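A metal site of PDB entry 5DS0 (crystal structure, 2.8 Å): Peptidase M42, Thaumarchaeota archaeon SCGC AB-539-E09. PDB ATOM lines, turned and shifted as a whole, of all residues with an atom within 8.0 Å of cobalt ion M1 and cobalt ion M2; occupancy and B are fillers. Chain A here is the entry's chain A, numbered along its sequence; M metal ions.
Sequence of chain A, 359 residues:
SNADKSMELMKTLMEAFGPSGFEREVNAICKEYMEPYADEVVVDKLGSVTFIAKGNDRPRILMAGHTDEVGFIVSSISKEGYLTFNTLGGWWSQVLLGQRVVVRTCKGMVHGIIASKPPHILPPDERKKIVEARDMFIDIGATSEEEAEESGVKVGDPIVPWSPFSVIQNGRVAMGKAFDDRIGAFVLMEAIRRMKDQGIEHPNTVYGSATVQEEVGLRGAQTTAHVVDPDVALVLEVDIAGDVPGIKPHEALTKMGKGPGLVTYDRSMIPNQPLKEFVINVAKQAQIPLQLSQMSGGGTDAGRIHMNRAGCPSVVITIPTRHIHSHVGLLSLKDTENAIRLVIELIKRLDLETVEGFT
Merely in contact with cobalt ion M2: Glu 214 (3.8 Å). Within 4 Å of cobalt ion M2: Asp 180, Glu 214, Glu 215 and His 325.
OD2 of Asp 180 is bound to cobalt ion M2 (1.8 Å). Cobalt ion M2 is bound by a ring nitrogen (NE2) of His 325. Cobalt ion M2 is bound by OE1 of Glu 215. The side-chain carboxylate (OE2) of Glu 215 binds cobalt ion M2, 2.3 Å away. Cobalt ion M2 has four donor atoms within binding distance.
Residues that only touch cobalt ion M1: Glu 214. Five residues have an atom within 4 Å of cobalt ion M1: His 66, Asp 180, Glu 214, Glu 215 and Glu 237.
The backbone NH of His 66 sits at hydrogen-bond distance from the side-chain carboxylate of Asp 181. The backbone NH (N) of Glu 214 is in hydrogen-bond range of the side-chain carboxylate (OD2) of Asp 68 (3.1 Å). The backbone NH of Glu 215 sits at hydrogen-bond distance from the side-chain carboxylate of Asp 68 (3.0 Å). O of Gly 90 sits at hydrogen-bond distance from ND1 of His 325, at 2.8 Å. OD1 of Asp 68 sits at hydrogen-bond distance from ND1 of His 66 (2.9 Å). NE2 of His 66 sits close to OE1 of Glu 214 (3.0 Å).
A ring nitrogen (NE2) of His 66 binds cobalt ion M1, at 2.0 Å. OD1 of Asp 180 is bound to cobalt ion M1, 2.0 Å away. OE2 of Glu 237 binds cobalt ion M1 (2.2 Å). OE1 of Glu 237 binds cobalt ion M1 (2.5 Å). Cobalt ion M1 has four donor atoms within binding distance.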
ATOM      1  N   GLY A  65      15.136   6.745   3.833  1.00  0.00           N
ATOM      2  CA  GLY A  65      14.052   7.725   3.999  1.00  0.00           C
ATOM      3  C   GLY A  65      14.092   8.253   5.421  1.00  0.00           C
ATOM      4  O   GLY A  65      14.091   7.477   6.357  1.00  0.00           O
ATOM      5  N   HIS A  66      14.133   9.561   5.584  1.00  0.00           N
ATOM      6  CA  HIS A  66      14.280  10.115   6.937  1.00  0.00           C
ATOM      7  C   HIS A  66      12.959  10.107   7.714  1.00  0.00           C
ATOM      8  O   HIS A  66      11.905  10.448   7.161  1.00  0.00           O
ATOM      9  CB  HIS A  66      14.920  11.510   6.913  1.00  0.00           C
ATOM     10  CG  HIS A  66      14.068  12.586   6.298  1.00  0.00           C
ATOM     11  ND1 HIS A  66      13.179  13.337   7.037  1.00  0.00           N
ATOM     12  CD2 HIS A  66      14.002  13.065   5.034  1.00  0.00           C
ATOM     13  CE1 HIS A  66      12.589  14.224   6.250  1.00  0.00           C
ATOM     14  NE2 HIS A  66      13.079  14.084   5.024  1.00  0.00           N
ATOM     15  N   THR A  67      13.022   9.713   8.971  1.00  0.00           N
ATOM     16  CA  THR A  67      11.855   9.646   9.804  1.00  0.00           C
ATOM     17  C   THR A  67      11.659  10.866  10.698  1.00  0.00           C
ATOM     18  O   THR A  67      10.633  10.977  11.383  1.00  0.00           O
ATOM     19  CB  THR A  67      11.910   8.443  10.739  1.00  0.00           C
ATOM     20  OG1 THR A  67      13.142   8.472  11.460  1.00  0.00           O
ATOM     21  CG2 THR A  67      11.802   7.160   9.933  1.00  0.00           C
ATOM     22  N   ASP A  68      12.631  11.771  10.724  1.00  0.00           N
ATOM     23  CA  ASP A  68      12.413  13.023  11.428  1.00  0.00           C
ATOM     24  C   ASP A  68      11.442  13.892  10.633  1.00  0.00           C
ATOM     25  O   ASP A  68      11.390  13.823   9.403  1.00  0.00           O
ATOM     26  CB  ASP A  68      13.725  13.763  11.751  1.00  0.00           C
ATOM     27  CG  ASP A  68      14.461  14.263  10.523  1.00  0.00           C
ATOM     28  OD1 ASP A  68      14.593  13.497   9.545  1.00  0.00           O
ATOM     29  OD2 ASP A  68      14.925  15.419  10.545  1.00  0.00           O
ATOM     30  N   GLU A  69      10.655  14.675  11.366  1.00  0.00           N
ATOM     31  CA  GLU A  69       9.711  15.636  10.775  1.00  0.00           C
ATOM     32  C   GLU A  69      10.060  17.021  11.261  1.00  0.00           C
ATOM     33  O   GLU A  69      10.685  17.220  12.304  1.00  0.00           O
ATOM     34  CB  GLU A  69       8.278  15.321  11.199  1.00  0.00           C
ATOM     35  CG  GLU A  69       8.089  15.320  12.717  1.00  0.00           C
ATOM     36  CD  GLU A  69       6.680  15.017  13.157  1.00  0.00           C
ATOM     37  OE1 GLU A  69       5.745  15.692  12.663  1.00  0.00           O
ATOM     38  OE2 GLU A  69       6.512  14.111  14.025  1.00  0.00           O
ATOM     39  N   VAL A  70       9.658  18.003  10.493  1.00  0.00           N
ATOM     40  CA  VAL A  70       9.843  19.369  10.962  1.00  0.00           C
ATOM     41  C   VAL A  70       9.045  19.529  12.227  1.00  0.00           C
ATOM     42  O   VAL A  70       7.994  18.919  12.384  1.00  0.00           O
ATOM     43  CB  VAL A  70       9.455  20.417   9.911  1.00  0.00           C
ATOM     44  CG1 VAL A  70      10.401  20.303   8.711  1.00  0.00           C
ATOM     45  CG2 VAL A  70       8.006  20.259   9.484  1.00  0.00           C
ATOM     46  N   GLY A  89      14.050  22.503  11.624  1.00  0.00           N
ATOM     47  CA  GLY A  89      13.833  22.312  10.193  1.00  0.00           C
ATOM     48  C   GLY A  89      13.186  23.560   9.630  1.00  0.00           C
ATOM     49  O   GLY A  89      12.810  24.464  10.381  1.00  0.00           O
ATOM     50  N   GLY A  90      13.076  23.619   8.317  1.00  0.00           N
ATOM     51  CA  GLY A  90      12.599  24.815   7.625  1.00  0.00           C
ATOM     52  C   GLY A  90      11.092  24.916   7.641  1.00  0.00           C
ATOM     53  O   GLY A  90      10.413  24.023   7.148  1.00  0.00           O
ATOM     54  N   PHE A 179       4.597  13.303   6.118  1.00  0.00           N
ATOM     55  CA  PHE A 179       4.845  12.510   4.911  1.00  0.00           C
ATOM     56  C   PHE A 179       6.302  12.638   4.519  1.00  0.00           C
ATOM     57  O   PHE A 179       6.918  11.671   4.129  1.00  0.00           O
ATOM     58  CB  PHE A 179       3.961  12.959   3.764  1.00  0.00           C
ATOM     59  CG  PHE A 179       2.520  12.581   3.920  1.00  0.00           C
ATOM     60  CD1 PHE A 179       2.153  11.307   4.297  1.00  0.00           C
ATOM     61  CD2 PHE A 179       1.521  13.518   3.683  1.00  0.00           C
ATOM     62  CE1 PHE A 179       0.825  10.979   4.453  1.00  0.00           C
ATOM     63  CE2 PHE A 179       0.176  13.180   3.836  1.00  0.00           C
ATOM     64  CZ  PHE A 179      -0.160  11.913   4.217  1.00  0.00           C
ATOM     65  N   ASP A 180       6.849  13.842   4.675  1.00  0.00           N
ATOM     66  CA  ASP A 180       8.267  14.087   4.501  1.00  0.00           C
ATOM     67  C   ASP A 180       8.947  13.729   5.827  1.00  0.00           C
ATOM     68  O   ASP A 180       8.891  14.509   6.752  1.00  0.00           O
ATOM     69  CB  ASP A 180       8.476  15.561   4.180  1.00  0.00           C
ATOM     70  CG  ASP A 180       9.926  15.949   4.007  1.00  0.00           C
ATOM     71  OD1 ASP A 180      10.797  15.053   3.872  1.00  0.00           O
ATOM     72  OD2 ASP A 180      10.194  17.168   3.993  1.00  0.00           O
ATOM     73  N   ASP A 181       9.608  12.573   5.939  1.00  0.00           N
ATOM     74  CA  ASP A 181       9.800  11.595   4.842  1.00  0.00           C
ATOM     75  C   ASP A 181       9.489  10.185   5.330  1.00  0.00           C
ATOM     76  O   ASP A 181      10.147   9.211   4.983  1.00  0.00           O
ATOM     77  CB  ASP A 181      11.241  11.683   4.313  1.00  0.00           C
ATOM     78  CG  ASP A 181      11.480  10.817   3.085  1.00  0.00           C
ATOM     79  OD1 ASP A 181      10.515  10.461   2.371  1.00  0.00           O
ATOM     80  OD2 ASP A 181      12.667  10.551   2.825  1.00  0.00           O
ATOM     81  N   ARG A 182       8.431  10.088   6.131  1.00  0.00           N
ATOM     82  CA  ARG A 182       8.013   8.809   6.639  1.00  0.00           C
ATOM     83  C   ARG A 182       7.364   7.989   5.523  1.00  0.00           C
ATOM     84  O   ARG A 182       7.354   6.756   5.591  1.00  0.00           O
ATOM     85  CB  ARG A 182       7.094   8.976   7.846  1.00  0.00           C
ATOM     86  CG  ARG A 182       7.890   9.390   9.075  1.00  0.00           C
ATOM     87  CD  ARG A 182       7.023   9.788  10.277  1.00  0.00           C
ATOM     88  NE  ARG A 182       7.796  10.611  11.214  1.00  0.00           N
ATOM     89  CZ  ARG A 182       7.292  11.236  12.264  1.00  0.00           C
ATOM     90  NH1 ARG A 182       5.997  11.117  12.554  1.00  0.00           N
ATOM     91  NH2 ARG A 182       8.073  11.966  13.050  1.00  0.00           N
ATOM     92  N   GLU A 214      17.492  14.652   9.045  1.00  0.00           N
ATOM     93  CA  GLU A 214      17.619  15.185   7.683  1.00  0.00           C
ATOM     94  C   GLU A 214      17.261  16.654   7.659  1.00  0.00           C
ATOM     95  O   GLU A 214      17.947  17.443   7.019  1.00  0.00           O
ATOM     96  CB  GLU A 214      16.699  14.450   6.689  1.00  0.00           C
ATOM     97  CG  GLU A 214      16.938  14.737   5.182  1.00  0.00           C
ATOM     98  CD  GLU A 214      16.172  15.938   4.588  1.00  0.00           C
ATOM     99  OE1 GLU A 214      15.053  16.313   5.039  1.00  0.00           O
ATOM    100  OE2 GLU A 214      16.694  16.518   3.608  1.00  0.00           O
ATOM    101  N   GLU A 215      16.174  17.005   8.345  1.00  0.00           N
ATOM    102  CA  GLU A 215      15.582  18.337   8.194  1.00  0.00           C
ATOM    103  C   GLU A 215      16.469  19.442   8.780  1.00  0.00           C
ATOM    104  O   GLU A 215      16.232  20.609   8.512  1.00  0.00           O
ATOM    105  CB  GLU A 215      14.169  18.400   8.778  1.00  0.00           C
ATOM    106  CG  GLU A 215      13.146  17.433   8.159  1.00  0.00           C
ATOM    107  CD  GLU A 215      12.552  17.855   6.804  1.00  0.00           C
ATOM    108  OE1 GLU A 215      11.397  17.490   6.471  1.00  0.00           O
ATOM    109  OE2 GLU A 215      13.238  18.549   6.054  1.00  0.00           O
ATOM    110  N   VAL A 216      17.494  19.069   9.541  1.00  0.00           N
ATOM    111  CA  VAL A 216      18.423  20.039  10.145  1.00  0.00           C
ATOM    112  C   VAL A 216      19.858  19.973   9.582  1.00  0.00           C
ATOM    113  O   VAL A 216      20.735  20.616  10.131  1.00  0.00           O
ATOM    114  CB  VAL A 216      18.499  19.923  11.699  1.00  0.00           C
ATOM    115  CG1 VAL A 216      17.149  20.235  12.336  1.00  0.00           C
ATOM    116  CG2 VAL A 216      18.995  18.552  12.156  1.00  0.00           C
ATOM    117  N   LEU A 218      21.068  16.949   7.026  1.00  0.00           N
ATOM    118  CA  LEU A 218      21.435  15.652   6.465  1.00  0.00           C
ATOM    119  C   LEU A 218      22.397  14.870   7.377  1.00  0.00           C
ATOM    120  O   LEU A 218      23.298  14.170   6.914  1.00  0.00           O
ATOM    121  CB  LEU A 218      22.042  15.838   5.067  1.00  0.00           C
ATOM    122  CG  LEU A 218      21.368  16.900   4.189  1.00  0.00           C
ATOM    123  CD1 LEU A 218      22.140  17.078   2.873  1.00  0.00           C
ATOM    124  CD2 LEU A 218      19.906  16.557   3.937  1.00  0.00           C
ATOM    125  N   VAL A 235      17.652   7.074  -2.680  1.00  0.00           N
ATOM    126  CA  VAL A 235      17.071   7.870  -1.639  1.00  0.00           C
ATOM    127  C   VAL A 235      15.630   8.134  -1.968  1.00  0.00           C
ATOM    128  O   VAL A 235      15.312   8.557  -3.077  1.00  0.00           O
ATOM    129  CB  VAL A 235      17.845   9.182  -1.459  1.00  0.00           C
ATOM    130  CG1 VAL A 235      17.098  10.112  -0.516  1.00  0.00           C
ATOM    131  CG2 VAL A 235      19.225   8.876  -0.917  1.00  0.00           C
ATOM    132  N   LEU A 236      14.758   7.899  -0.997  1.00  0.00           N
ATOM    133  CA  LEU A 236      13.337   8.124  -1.159  1.00  0.00           C
ATOM    134  C   LEU A 236      12.944   9.371  -0.405  1.00  0.00           C
ATOM    135  O   LEU A 236      13.235   9.502   0.764  1.00  0.00           O
ATOM    136  CB  LEU A 236      12.556   6.943  -0.626  1.00  0.00           C
ATOM    137  CG  LEU A 236      12.920   5.698  -1.412  1.00  0.00           C
ATOM    138  CD1 LEU A 236      12.740   4.413  -0.630  1.00  0.00           C
ATOM    139  CD2 LEU A 236      12.098   5.653  -2.674  1.00  0.00           C
ATOM    140  N   GLU A 237      12.289  10.291  -1.103  1.00  0.00           N
ATOM    141  CA  GLU A 237      11.910  11.567  -0.538  1.00  0.00           C
ATOM    142  C   GLU A 237      10.544  11.942  -1.071  1.00  0.00           C
ATOM    143  O   GLU A 237       9.928  11.204  -1.828  1.00  0.00           O
ATOM    144  CB  GLU A 237      12.924  12.661  -0.926  1.00  0.00           C
ATOM    145  CG  GLU A 237      13.908  13.099   0.156  1.00  0.00           C
ATOM    146  CD  GLU A 237      13.318  13.825   1.364  1.00  0.00           C
ATOM    147  OE1 GLU A 237      12.102  14.061   1.468  1.00  0.00           O
ATOM    148  OE2 GLU A 237      14.119  14.163   2.260  1.00  0.00           O
ATOM    149  N   VAL A 238      10.066  13.099  -0.640  1.00  0.00           N
ATOM    150  CA  VAL A 238       8.882  13.699  -1.201  1.00  0.00           C
ATOM    151  C   VAL A 238       9.323  14.726  -2.227  1.00  0.00           C
ATOM    152  O   VAL A 238      10.451  15.195  -2.200  1.00  0.00           O
ATOM    153  CB  VAL A 238       8.008  14.357  -0.134  1.00  0.00           C
ATOM    154  CG1 VAL A 238       7.446  13.308   0.804  1.00  0.00           C
ATOM    155  CG2 VAL A 238       8.802  15.402   0.648  1.00  0.00           C
ATOM    156  N   ASP A 239       8.427  15.061  -3.136  1.00  0.00           N
ATOM    157  CA  ASP A 239       8.649  16.108  -4.086  1.00  0.00           C
ATOM    158  C   ASP A 239       7.578  17.146  -3.820  1.00  0.00           C
ATOM    159  O   ASP A 239       6.432  16.790  -3.504  1.00  0.00           O
ATOM    160  CB  ASP A 239       8.504  15.562  -5.519  1.00  0.00           C
ATOM    161  CG  ASP A 239       9.600  16.052  -6.478  1.00  0.00           C
ATOM    162  OD1 ASP A 239       9.992  17.245  -6.397  1.00  0.00           O
ATOM    163  OD2 ASP A 239      10.066  15.226  -7.306  1.00  0.00           O
ATOM    164  N   ILE A 240       7.928  18.408  -3.941  1.00  0.00           N
ATOM    165  CA  ILE A 240       6.922  19.445  -3.848  1.00  0.00           C
ATOM    166  C   ILE A 240       6.050  19.341  -5.098  1.00  0.00           C
ATOM    167  O   ILE A 240       6.550  19.435  -6.206  1.00  0.00           O
ATOM    168  CB  ILE A 240       7.529  20.853  -3.766  1.00  0.00           C
ATOM    169  CG1 ILE A 240       8.360  21.033  -2.486  1.00  0.00           C
ATOM    170  CG2 ILE A 240       6.426  21.907  -3.809  1.00  0.00           C
ATOM    171  CD1 ILE A 240       9.858  21.022  -2.696  1.00  0.00           C
ATOM    172  N   GLY A 299      17.603  20.007  -0.784  1.00  0.00           N
ATOM    173  CA  GLY A 299      18.530  18.879  -0.762  1.00  0.00           C
ATOM    174  C   GLY A 299      17.925  17.643  -0.129  1.00  0.00           C
ATOM    175  O   GLY A 299      16.786  17.671   0.337  1.00  0.00           O
ATOM    176  N   THR A 300      18.710  16.559  -0.125  1.00  0.00           N
ATOM    177  CA  THR A 300      18.266  15.231   0.315  1.00  0.00           C
ATOM    178  C   THR A 300      19.375  14.491   1.051  1.00  0.00           C
ATOM    179  O   THR A 300      20.534  14.904   0.992  1.00  0.00           O
ATOM    180  CB  THR A 300      17.864  14.347  -0.876  1.00  0.00           C
ATOM    181  OG1 THR A 300      18.952  14.288  -1.812  1.00  0.00           O
ATOM    182  CG2 THR A 300      16.652  14.921  -1.561  1.00  0.00           C
ATOM    183  N   ASP A 301      19.023  13.410   1.734  1.00  0.00           N
ATOM    184  CA  ASP A 301      20.017  12.514   2.346  1.00  0.00           C
ATOM    185  C   ASP A 301      21.112  12.164   1.317  1.00  0.00           C
ATOM    186  O   ASP A 301      22.274  11.949   1.695  1.00  0.00           O
ATOM    187  CB  ASP A 301      19.388  11.202   2.821  1.00  0.00           C
ATOM    188  CG  ASP A 301      18.523  11.353   4.089  1.00  0.00           C
ATOM    189  OD1 ASP A 301      18.911  12.106   5.023  1.00  0.00           O
ATOM    190  OD2 ASP A 301      17.473  10.651   4.126  1.00  0.00           O
ATOM    191  N   ILE A 324       4.070  20.071   1.988  1.00  0.00           N
ATOM    192  CA  ILE A 324       5.070  19.553   2.925  1.00  0.00           C
ATOM    193  C   ILE A 324       5.566  20.660   3.852  1.00  0.00           C
ATOM    194  O   ILE A 324       5.251  21.834   3.643  1.00  0.00           O
ATOM    195  CB  ILE A 324       6.270  18.928   2.211  1.00  0.00           C
ATOM    196  CG1 ILE A 324       7.002  19.958   1.361  1.00  0.00           C
ATOM    197  CG2 ILE A 324       5.804  17.763   1.353  1.00  0.00           C
ATOM    198  CD1 ILE A 324       8.395  19.513   0.939  1.00  0.00           C
ATOM    199  N   HIS A 325       6.301  20.286   4.886  1.00  0.00           N
ATOM    200  CA  HIS A 325       6.791  21.238   5.883  1.00  0.00           C
ATOM    201  C   HIS A 325       5.657  22.124   6.405  1.00  0.00           C
ATOM    202  O   HIS A 325       5.821  23.334   6.600  1.00  0.00           O
ATOM    203  CB  HIS A 325       7.925  22.091   5.300  1.00  0.00           C
ATOM    204  CG  HIS A 325       9.207  21.345   5.109  1.00  0.00           C
ATOM    205  ND1 HIS A 325      10.435  21.937   5.312  1.00  0.00           N
ATOM    206  CD2 HIS A 325       9.455  20.067   4.754  1.00  0.00           C
ATOM    207  CE1 HIS A 325      11.386  21.044   5.079  1.00  0.00           C
ATOM    208  NE2 HIS A 325      10.818  19.906   4.743  1.00  0.00           N
HETATM  209 CO    CO M   1      12.769  15.311   3.487  1.00  0.00          CO
HETATM  210 CO    CO M   2      11.767  18.071   4.306  1.00  0.00          CO
